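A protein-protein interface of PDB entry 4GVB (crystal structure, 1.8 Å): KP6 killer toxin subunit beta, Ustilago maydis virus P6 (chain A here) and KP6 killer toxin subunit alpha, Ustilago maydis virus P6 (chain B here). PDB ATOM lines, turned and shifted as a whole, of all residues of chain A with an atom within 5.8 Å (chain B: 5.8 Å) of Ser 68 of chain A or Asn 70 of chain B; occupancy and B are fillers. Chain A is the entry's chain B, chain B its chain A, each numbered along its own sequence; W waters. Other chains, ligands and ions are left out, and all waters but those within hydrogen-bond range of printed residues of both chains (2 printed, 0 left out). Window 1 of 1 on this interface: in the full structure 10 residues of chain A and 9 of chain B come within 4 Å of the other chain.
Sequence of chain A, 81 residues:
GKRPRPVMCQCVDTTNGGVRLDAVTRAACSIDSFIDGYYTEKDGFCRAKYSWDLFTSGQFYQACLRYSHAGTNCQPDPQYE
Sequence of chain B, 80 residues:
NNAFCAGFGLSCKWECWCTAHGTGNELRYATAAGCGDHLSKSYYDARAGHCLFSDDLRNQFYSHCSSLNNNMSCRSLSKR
The side-chain amide oxygen (OD1) of Asn 70 of chain B sits at hydrogen-bond distance from the side-chain hydroxyl (OG) of Ser 68 of chain A (3.3 Å).
The side-chain hydroxyl (OG) of Ser 68 of chain A sits at hydrogen-bond distance from the backbone carbonyl oxygen (O) of Leu 68 of chain B, at 2.7 Å.
The backbone carbonyl oxygen of Tyr 67 of chain A is in hydrogen-bond range of the side-chain amide nitrogen of Asn 70 of chain B.
The side-chain amide oxygen (OD1) of Asn 70 of chain B lies close to the backbone carbonyl oxygen (O) of Leu 68 of chain B (3.5 Å).
The backbone NH (N) of Leu 27 of chain B is in hydrogen-bond range of the backbone carbonyl oxygen (O) of Cys 18 of chain B, at 3.1 Å.
O of Cys 65 of chain B lies within hydrogen-bond range of N of Asn 70 of chain B.
The side-chain sulfur (SG) of Cys 65 of chain B forms a disulfide with the side-chain sulfur (SG) of Cys 18 of chain B (2.0 Å).
Among the printed residues, pairs that only touch across the chains: Leu 21 of chain A with Asn 69 of chain B (3.7 Å), Val 24 of chain A with Leu 68 of chain B (3.4 Å), Leu 65 of chain A with Leu 27 of chain B (3.7 Å), Arg 66 of chain A with Ala 30 of chain B (3.8 Å), Tyr 67 of chain A with Ala 30 of chain B (3.8 Å), Tyr 67 of chain A with Leu 68 of chain B (3.8 Å), Ser 68 of chain A with Asn 69 of chain B (3.5 Å), His 69 of chain A with Ala 20 of chain B (3.9 Å), His 69 of chain A with His 21 of chain B (3.5 Å) and His 69 of chain A with Asn 70 of chain B (3.9 Å).
Of the printed residues of chain B, Tyr 67 of chain A touches Ala 30 (3.8 Å), Leu 68 (3.8 Å) and Asn 70 (2.8 Å).
Ser 68 of chain A touches three residues of chain B.
Printed residues of chain B within 4 Å of His 69 of chain A: Ala 20, His 21 and Asn 70.
Asn 70 of chain B touches just these residues of chain A: Tyr 67 (2.8 Å), Ser 68 (3.3 Å) and His 69 (3.9 Å).
The nearest residue of chain B that does not touch Ser 68 of chain A is Leu 27 of chain B (4.1 Å).
The nearest printed residue of chain A that does not touch Asn 70 of chain B is Arg 66 of chain A (6.3 Å).
The nearest printed residue of chain B that does not touch Tyr 67 of chain A is Leu 27 of chain B (4.2 Å).
Of the 10 printed residues of chain A, 7 touch a printed residue of chain B.
Hydrophobic or aromatic side chains of chain A that line the printed part of chain B: Leu 21, Val 24, Tyr 67 and His 69.
Hydrophobic or aromatic side chains of chain B that line the printed part of chain A: Ala 20, His 21, Leu 27, Ala 30 and Leu 68.
Among the printed residues, 13 pairs touch across the chains.
Water W2 lies within hydrogen-bond range of the side-chain amide nitrogen (ND2) of Asn 69 of chain B, the side-chain hydroxyl (OG) of Ser 68 of chain A, the backbone carbonyl oxygen (O) of His 69 of chain A and a ring nitrogen (ND1) of His 21 of chain B.
Water W1 lies within hydrogen-bond range of the side-chain amide oxygen (OD1) of Asn 70 of chain B (2.7 Å), the backbone NH (N) of His 69 of chain A (2.9 Å), the backbone NH (N) of His 21 of chain B (3.0 Å), the backbone carbonyl oxygen (O) of Asn 69 of chain B (3.0 Å) and the side-chain hydroxyl (OG) of Ser 68 of chain A (3.4 Å).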
ATOM      1  N   LEU A  21       1.176 -16.336 -15.354  1.00  0.00           N
ATOM      2  CA  LEU A  21       0.713 -16.691 -16.700  1.00  0.00           C
ATOM      3  C   LEU A  21       0.466 -15.388 -17.418  1.00  0.00           C
ATOM      4  O   LEU A  21      -0.626 -14.823 -17.341  1.00  0.00           O
ATOM      5  CB  LEU A  21      -0.583 -17.504 -16.636  1.00  0.00           C
ATOM      6  CG  LEU A  21      -0.560 -18.861 -15.933  1.00  0.00           C
ATOM      7  CD1 LEU A  21      -1.967 -19.497 -15.882  1.00  0.00           C
ATOM      8  CD2 LEU A  21       0.434 -19.770 -16.592  1.00  0.00           C
ATOM      9  N   VAL A  24      -2.464 -14.586 -19.903  1.00  0.00           N
ATOM     10  CA  VAL A  24      -3.722 -14.631 -19.165  1.00  0.00           C
ATOM     11  C   VAL A  24      -3.905 -13.319 -18.400  1.00  0.00           C
ATOM     12  O   VAL A  24      -4.969 -12.694 -18.433  1.00  0.00           O
ATOM     13  CB  VAL A  24      -3.748 -15.843 -18.195  1.00  0.00           C
ATOM     14  CG1 VAL A  24      -5.088 -15.933 -17.504  1.00  0.00           C
ATOM     15  CG2 VAL A  24      -3.474 -17.146 -18.963  1.00  0.00           C
ATOM     16  N   ALA A  63     -11.824 -12.213 -13.669  1.00  0.00           N
ATOM     17  CA  ALA A  63     -11.186 -11.951 -14.966  1.00  0.00           C
ATOM     18  C   ALA A  63     -10.212 -13.063 -15.371  1.00  0.00           C
ATOM     19  O   ALA A  63     -10.277 -13.592 -16.484  1.00  0.00           O
ATOM     20  CB  ALA A  63     -10.482 -10.597 -14.956  1.00  0.00           C
ATOM     21  N   CYS A  64      -9.312 -13.421 -14.460  1.00  0.00           N
ATOM     22  CA  CYS A  64      -8.357 -14.494 -14.719  1.00  0.00           C
ATOM     23  C   CYS A  64      -9.080 -15.787 -15.089  1.00  0.00           C
ATOM     24  O   CYS A  64      -8.705 -16.462 -16.039  1.00  0.00           O
ATOM     25  CB  CYS A  64      -7.451 -14.739 -13.506  1.00  0.00           C
ATOM     26  SG  CYS A  64      -6.329 -13.362 -13.126  1.00  0.00           S
ATOM     27  N   LEU A  65     -10.122 -16.117 -14.335  1.00  0.00           N
ATOM     28  CA  LEU A  65     -10.828 -17.377 -14.510  1.00  0.00           C
ATOM     29  C   LEU A  65     -11.620 -17.444 -15.814  1.00  0.00           C
ATOM     30  O   LEU A  65     -11.957 -18.526 -16.279  1.00  0.00           O
ATOM     31  CB  LEU A  65     -11.744 -17.653 -13.320  1.00  0.00           C
ATOM     32  CG  LEU A  65     -11.116 -18.352 -12.117  1.00  0.00           C
ATOM     33  CD1 LEU A  65     -12.188 -18.596 -11.072  1.00  0.00           C
ATOM     34  CD2 LEU A  65     -10.465 -19.675 -12.530  1.00  0.00           C
ATOM     35  N   ARG A  66     -11.927 -16.292 -16.390  1.00  0.00           N
ATOM     36  CA  ARG A  66     -12.574 -16.265 -17.695  1.00  0.00           C
ATOM     37  C   ARG A  66     -11.625 -16.705 -18.809  1.00  0.00           C
ATOM     38  O   ARG A  66     -12.069 -17.131 -19.884  1.00  0.00           O
ATOM     39  CB  ARG A  66     -13.139 -14.878 -17.982  1.00  0.00           C
ATOM     40  CG  ARG A  66     -14.513 -14.679 -17.367  1.00  0.00           C
ATOM     41  CD  ARG A  66     -14.606 -13.363 -16.654  1.00  0.00           C
ATOM     42  NE  ARG A  66     -14.667 -12.246 -17.592  1.00  0.00           N
ATOM     43  CZ  ARG A  66     -15.759 -11.524 -17.813  1.00  0.00           C
ATOM     44  NH1 ARG A  66     -16.877 -11.800 -17.159  1.00  0.00           N
ATOM     45  NH2 ARG A  66     -15.733 -10.522 -18.681  1.00  0.00           N
ATOM     46  N   TYR A  67     -10.322 -16.630 -18.553  1.00  0.00           N
ATOM     47  CA  TYR A  67      -9.359 -16.892 -19.620  1.00  0.00           C
ATOM     48  C   TYR A  67      -8.528 -18.155 -19.478  1.00  0.00           C
ATOM     49  O   TYR A  67      -7.982 -18.646 -20.463  1.00  0.00           O
ATOM     50  CB  TYR A  67      -8.469 -15.660 -19.884  1.00  0.00           C
ATOM     51  CG  TYR A  67      -9.255 -14.541 -20.519  1.00  0.00           C
ATOM     52  CD1 TYR A  67      -9.507 -14.538 -21.889  1.00  0.00           C
ATOM     53  CD2 TYR A  67      -9.781 -13.512 -19.753  1.00  0.00           C
ATOM     54  CE1 TYR A  67     -10.249 -13.541 -22.469  1.00  0.00           C
ATOM     55  CE2 TYR A  67     -10.525 -12.506 -20.333  1.00  0.00           C
ATOM     56  CZ  TYR A  67     -10.753 -12.530 -21.692  1.00  0.00           C
ATOM     57  OH  TYR A  67     -11.494 -11.530 -22.274  1.00  0.00           O
ATOM     58  N   SER A  68      -8.445 -18.689 -18.262  1.00  0.00           N
ATOM     59  CA  SER A  68      -7.623 -19.864 -18.002  1.00  0.00           C
ATOM     60  C   SER A  68      -8.000 -20.508 -16.676  1.00  0.00           C
ATOM     61  O   SER A  68      -8.684 -19.894 -15.852  1.00  0.00           O
ATOM     62  CB  SER A  68      -6.143 -19.464 -17.976  1.00  0.00           C
ATOM     63  OG  SER A  68      -5.288 -20.598 -18.055  1.00  0.00           O
ATOM     64  N   HIS A  69      -7.560 -21.744 -16.450  1.00  0.00           N
ATOM     65  CA  HIS A  69      -7.733 -22.305 -15.117  1.00  0.00           C
ATOM     66  C   HIS A  69      -6.648 -21.707 -14.234  1.00  0.00           C
ATOM     67  O   HIS A  69      -5.578 -22.301 -14.040  1.00  0.00           O
ATOM     68  CB  HIS A  69      -7.640 -23.822 -15.088  1.00  0.00           C
ATOM     69  CG  HIS A  69      -7.952 -24.406 -13.740  1.00  0.00           C
ATOM     70  ND1 HIS A  69      -9.208 -24.349 -13.179  1.00  0.00           N
ATOM     71  CD2 HIS A  69      -7.166 -25.028 -12.830  1.00  0.00           C
ATOM     72  CE1 HIS A  69      -9.190 -24.923 -11.993  1.00  0.00           C
ATOM     73  NE2 HIS A  69      -7.960 -25.342 -11.755  1.00  0.00           N
ATOM     74  N   ALA A  70      -6.922 -20.514 -13.723  1.00  0.00           N
ATOM     75  CA  ALA A  70      -5.891 -19.751 -13.042  1.00  0.00           C
ATOM     76  C   ALA A  70      -6.363 -19.232 -11.692  1.00  0.00           C
ATOM     77  O   ALA A  70      -7.560 -19.094 -11.439  1.00  0.00           O
ATOM     78  CB  ALA A  70      -5.435 -18.588 -13.919  1.00  0.00           C
ATOM     79  N   CYS B  18     -11.518 -23.429 -26.550  1.00  0.00           N
ATOM     80  CA  CYS B  18     -10.519 -23.526 -25.493  1.00  0.00           C
ATOM     81  C   CYS B  18     -11.104 -24.246 -24.274  1.00  0.00           C
ATOM     82  O   CYS B  18     -12.264 -24.057 -23.947  1.00  0.00           O
ATOM     83  CB  CYS B  18     -10.040 -22.128 -25.093  1.00  0.00           C
ATOM     84  SG  CYS B  18      -9.211 -21.230 -26.424  1.00  0.00           S
ATOM     85  N   THR B  19     -10.290 -25.067 -23.613  1.00  0.00           N
ATOM     86  CA  THR B  19     -10.715 -25.772 -22.407  1.00  0.00           C
ATOM     87  C   THR B  19      -9.752 -25.572 -21.244  1.00  0.00           C
ATOM     88  O   THR B  19      -8.543 -25.562 -21.421  1.00  0.00           O
ATOM     89  CB  THR B  19     -10.904 -27.280 -22.656  1.00  0.00           C
ATOM     90  OG1 THR B  19      -9.666 -27.865 -23.070  1.00  0.00           O
ATOM     91  CG2 THR B  19     -11.954 -27.512 -23.729  1.00  0.00           C
ATOM     92  N   ALA B  20     -10.301 -25.386 -20.054  1.00  0.00           N
ATOM     93  CA  ALA B  20      -9.484 -25.259 -18.851  1.00  0.00           C
ATOM     94  C   ALA B  20      -8.780 -26.577 -18.590  1.00  0.00           C
ATOM     95  O   ALA B  20      -9.402 -27.641 -18.658  1.00  0.00           O
ATOM     96  CB  ALA B  20     -10.346 -24.888 -17.686  1.00  0.00           C
ATOM     97  N   HIS B  21      -7.480 -26.533 -18.323  1.00  0.00           N
ATOM     98  CA  HIS B  21      -6.782 -27.765 -17.983  1.00  0.00           C
ATOM     99  C   HIS B  21      -7.380 -28.356 -16.693  1.00  0.00           C
ATOM    100  O   HIS B  21      -7.961 -27.633 -15.883  1.00  0.00           O
ATOM    101  CB  HIS B  21      -5.266 -27.549 -17.887  1.00  0.00           C
ATOM    102  CG  HIS B  21      -4.818 -26.854 -16.636  1.00  0.00           C
ATOM    103  ND1 HIS B  21      -3.964 -25.771 -16.652  1.00  0.00           N
ATOM    104  CD2 HIS B  21      -5.084 -27.103 -15.331  1.00  0.00           C
ATOM    105  CE1 HIS B  21      -3.729 -25.377 -15.409  1.00  0.00           C
ATOM    106  NE2 HIS B  21      -4.399 -26.169 -14.589  1.00  0.00           N
ATOM    107  N   LEU B  27     -14.057 -22.534 -22.003  1.00  0.00           N
ATOM    108  CA  LEU B  27     -13.767 -21.146 -21.652  1.00  0.00           C
ATOM    109  C   LEU B  27     -14.140 -20.195 -22.786  1.00  0.00           C
ATOM    110  O   LEU B  27     -13.301 -19.850 -23.631  1.00  0.00           O
ATOM    111  CB  LEU B  27     -12.292 -20.990 -21.280  1.00  0.00           C
ATOM    112  CG  LEU B  27     -11.873 -21.855 -20.087  1.00  0.00           C
ATOM    113  CD1 LEU B  27     -10.361 -22.083 -20.072  1.00  0.00           C
ATOM    114  CD2 LEU B  27     -12.354 -21.191 -18.801  1.00  0.00           C
ATOM    115  N   ALA B  30     -12.074 -17.061 -23.682  1.00  0.00           N
ATOM    116  CA  ALA B  30     -10.806 -17.371 -24.327  1.00  0.00           C
ATOM    117  C   ALA B  30     -11.049 -17.766 -25.789  1.00  0.00           C
ATOM    118  O   ALA B  30     -10.318 -17.358 -26.694  1.00  0.00           O
ATOM    119  CB  ALA B  30     -10.108 -18.488 -23.597  1.00  0.00           C
ATOM    120  N   TYR B  62      -5.233 -23.370 -31.949  1.00  0.00           N
ATOM    121  CA  TYR B  62      -4.558 -24.045 -30.848  1.00  0.00           C
ATOM    122  C   TYR B  62      -3.513 -23.156 -30.200  1.00  0.00           C
ATOM    123  O   TYR B  62      -3.326 -23.189 -28.979  1.00  0.00           O
ATOM    124  CB  TYR B  62      -3.875 -25.332 -31.311  1.00  0.00           C
ATOM    125  CG  TYR B  62      -3.057 -25.958 -30.185  1.00  0.00           C
ATOM    126  CD1 TYR B  62      -3.673 -26.685 -29.173  1.00  0.00           C
ATOM    127  CD2 TYR B  62      -1.680 -25.798 -30.127  1.00  0.00           C
ATOM    128  CE1 TYR B  62      -2.926 -27.254 -28.140  1.00  0.00           C
ATOM    129  CE2 TYR B  62      -0.933 -26.354 -29.098  1.00  0.00           C
ATOM    130  CZ  TYR B  62      -1.565 -27.077 -28.114  1.00  0.00           C
ATOM    131  OH  TYR B  62      -0.820 -27.627 -27.101  1.00  0.00           O
ATOM    132  N   CYS B  65      -5.359 -20.858 -27.750  1.00  0.00           N
ATOM    133  CA  CYS B  65      -5.760 -21.532 -26.510  1.00  0.00           C
ATOM    134  C   CYS B  65      -4.531 -21.832 -25.671  1.00  0.00           C
ATOM    135  O   CYS B  65      -4.531 -21.602 -24.460  1.00  0.00           O
ATOM    136  CB  CYS B  65      -6.523 -22.831 -26.789  1.00  0.00           C
ATOM    137  SG  CYS B  65      -8.144 -22.553 -27.524  1.00  0.00           S
ATOM    138  N   SER B  66      -3.490 -22.341 -26.324  1.00  0.00           N
ATOM    139  CA  SER B  66      -2.248 -22.701 -25.649  1.00  0.00           C
ATOM    140  C   SER B  66      -1.492 -21.502 -25.058  1.00  0.00           C
ATOM    141  O   SER B  66      -0.857 -21.625 -23.999  1.00  0.00           O
ATOM    142  CB  SER B  66      -1.343 -23.487 -26.600  1.00  0.00           C
ATOM    143  OG  SER B  66      -0.058 -23.669 -26.033  1.00  0.00           O
ATOM    144  N   SER B  67      -1.559 -20.353 -25.730  1.00  0.00           N
ATOM    145  CA  SER B  67      -0.940 -19.129 -25.207  1.00  0.00           C
ATOM    146  C   SER B  67      -1.562 -18.716 -23.871  1.00  0.00           C
ATOM    147  O   SER B  67      -0.916 -18.056 -23.031  1.00  0.00           O
ATOM    148  CB  SER B  67      -1.049 -17.973 -26.214  1.00  0.00           C
ATOM    149  OG  SER B  67      -2.355 -17.387 -26.251  1.00  0.00           O
ATOM    150  N   LEU B  68      -2.817 -19.117 -23.674  1.00  0.00           N
ATOM    151  CA  LEU B  68      -3.558 -18.812 -22.448  1.00  0.00           C
ATOM    152  C   LEU B  68      -3.539 -19.966 -21.442  1.00  0.00           C
ATOM    153  O   LEU B  68      -4.362 -20.011 -20.532  1.00  0.00           O
ATOM    154  CB  LEU B  68      -5.008 -18.430 -22.773  1.00  0.00           C
ATOM    155  CG  LEU B  68      -5.192 -17.096 -23.491  1.00  0.00           C
ATOM    156  CD1 LEU B  68      -6.658 -16.907 -23.880  1.00  0.00           C
ATOM    157  CD2 LEU B  68      -4.693 -15.943 -22.618  1.00  0.00           C
ATOM    158  N   ASN B  69      -2.586 -20.874 -21.616  1.00  0.00           N
ATOM    159  CA  ASN B  69      -2.418 -22.031 -20.739  1.00  0.00           C
ATOM    160  C   ASN B  69      -3.594 -22.990 -20.793  1.00  0.00           C
ATOM    161  O   ASN B  69      -3.871 -23.700 -19.824  1.00  0.00           O
ATOM    162  CB  ASN B  69      -2.169 -21.590 -19.294  1.00  0.00           C
ATOM    163  CG  ASN B  69      -1.318 -22.581 -18.525  1.00  0.00           C
ATOM    164  OD1 ASN B  69      -0.307 -23.077 -19.031  1.00  0.00           O
ATOM    165  ND2 ASN B  69      -1.731 -22.887 -17.306  1.00  0.00           N
ATOM    166  N   ASN B  70      -4.287 -23.023 -21.928  1.00  0.00           N
ATOM    167  CA  ASN B  70      -5.453 -23.892 -22.055  1.00  0.00           C
ATOM    168  C   ASN B  70      -5.230 -25.041 -23.031  1.00  0.00           C
ATOM    169  O   ASN B  70      -4.254 -25.066 -23.779  1.00  0.00           O
ATOM    170  CB  ASN B  70      -6.682 -23.101 -22.507  1.00  0.00           C
ATOM    171  CG  ASN B  70      -7.088 -22.036 -21.527  1.00  0.00           C
ATOM    172  OD1 ASN B  70      -7.027 -22.231 -20.315  1.00  0.00           O
ATOM    173  ND2 ASN B  70      -7.511 -20.895 -22.047  1.00  0.00           N
ATOM    174  N   ASN B  71      -6.154 -25.993 -23.016  1.00  0.00           N
ATOM    175  CA  ASN B  71      -6.179 -27.029 -24.041  1.00  0.00           C
ATOM    176  C   ASN B  71      -7.168 -26.645 -25.140  1.00  0.00           C
ATOM    177  O   ASN B  71      -7.818 -25.595 -25.063  1.00  0.00           O
ATOM    178  CB  ASN B  71      -6.554 -28.384 -23.433  1.00  0.00           C
ATOM    179  CG  ASN B  71      -5.529 -28.872 -22.402  1.00  0.00           C
ATOM    180  OD1 ASN B  71      -5.896 -29.372 -21.335  1.00  0.00           O
ATOM    181  ND2 ASN B  71      -4.243 -28.724 -22.719  1.00  0.00           N
ATOM    182  N   MET B  72      -7.286 -27.482 -26.168  1.00  0.00           N
ATOM    183  CA  MET B  72      -8.288 -27.232 -27.201  1.00  0.00           C
ATOM    184  C   MET B  72      -9.076 -28.500 -27.516  1.00  0.00           C
ATOM    185  O   MET B  72      -8.507 -29.577 -27.622  1.00  0.00           O
ATOM    186  CB  MET B  72      -7.627 -26.720 -28.475  1.00  0.00           C
ATOM    187  CG  MET B  72      -8.600 -26.573 -29.636  1.00  0.00           C
ATOM    188  SD  MET B  72      -7.736 -26.133 -31.151  1.00  0.00           S
ATOM    189  CE  MET B  72      -6.897 -27.668 -31.538  1.00  0.00           C
HETATM  190  O   HOH W   1      -6.411 -23.764 -18.242  1.00  0.00           O
HETATM  191  O   HOH W   2      -4.104 -22.421 -16.384  1.00  0.00           O
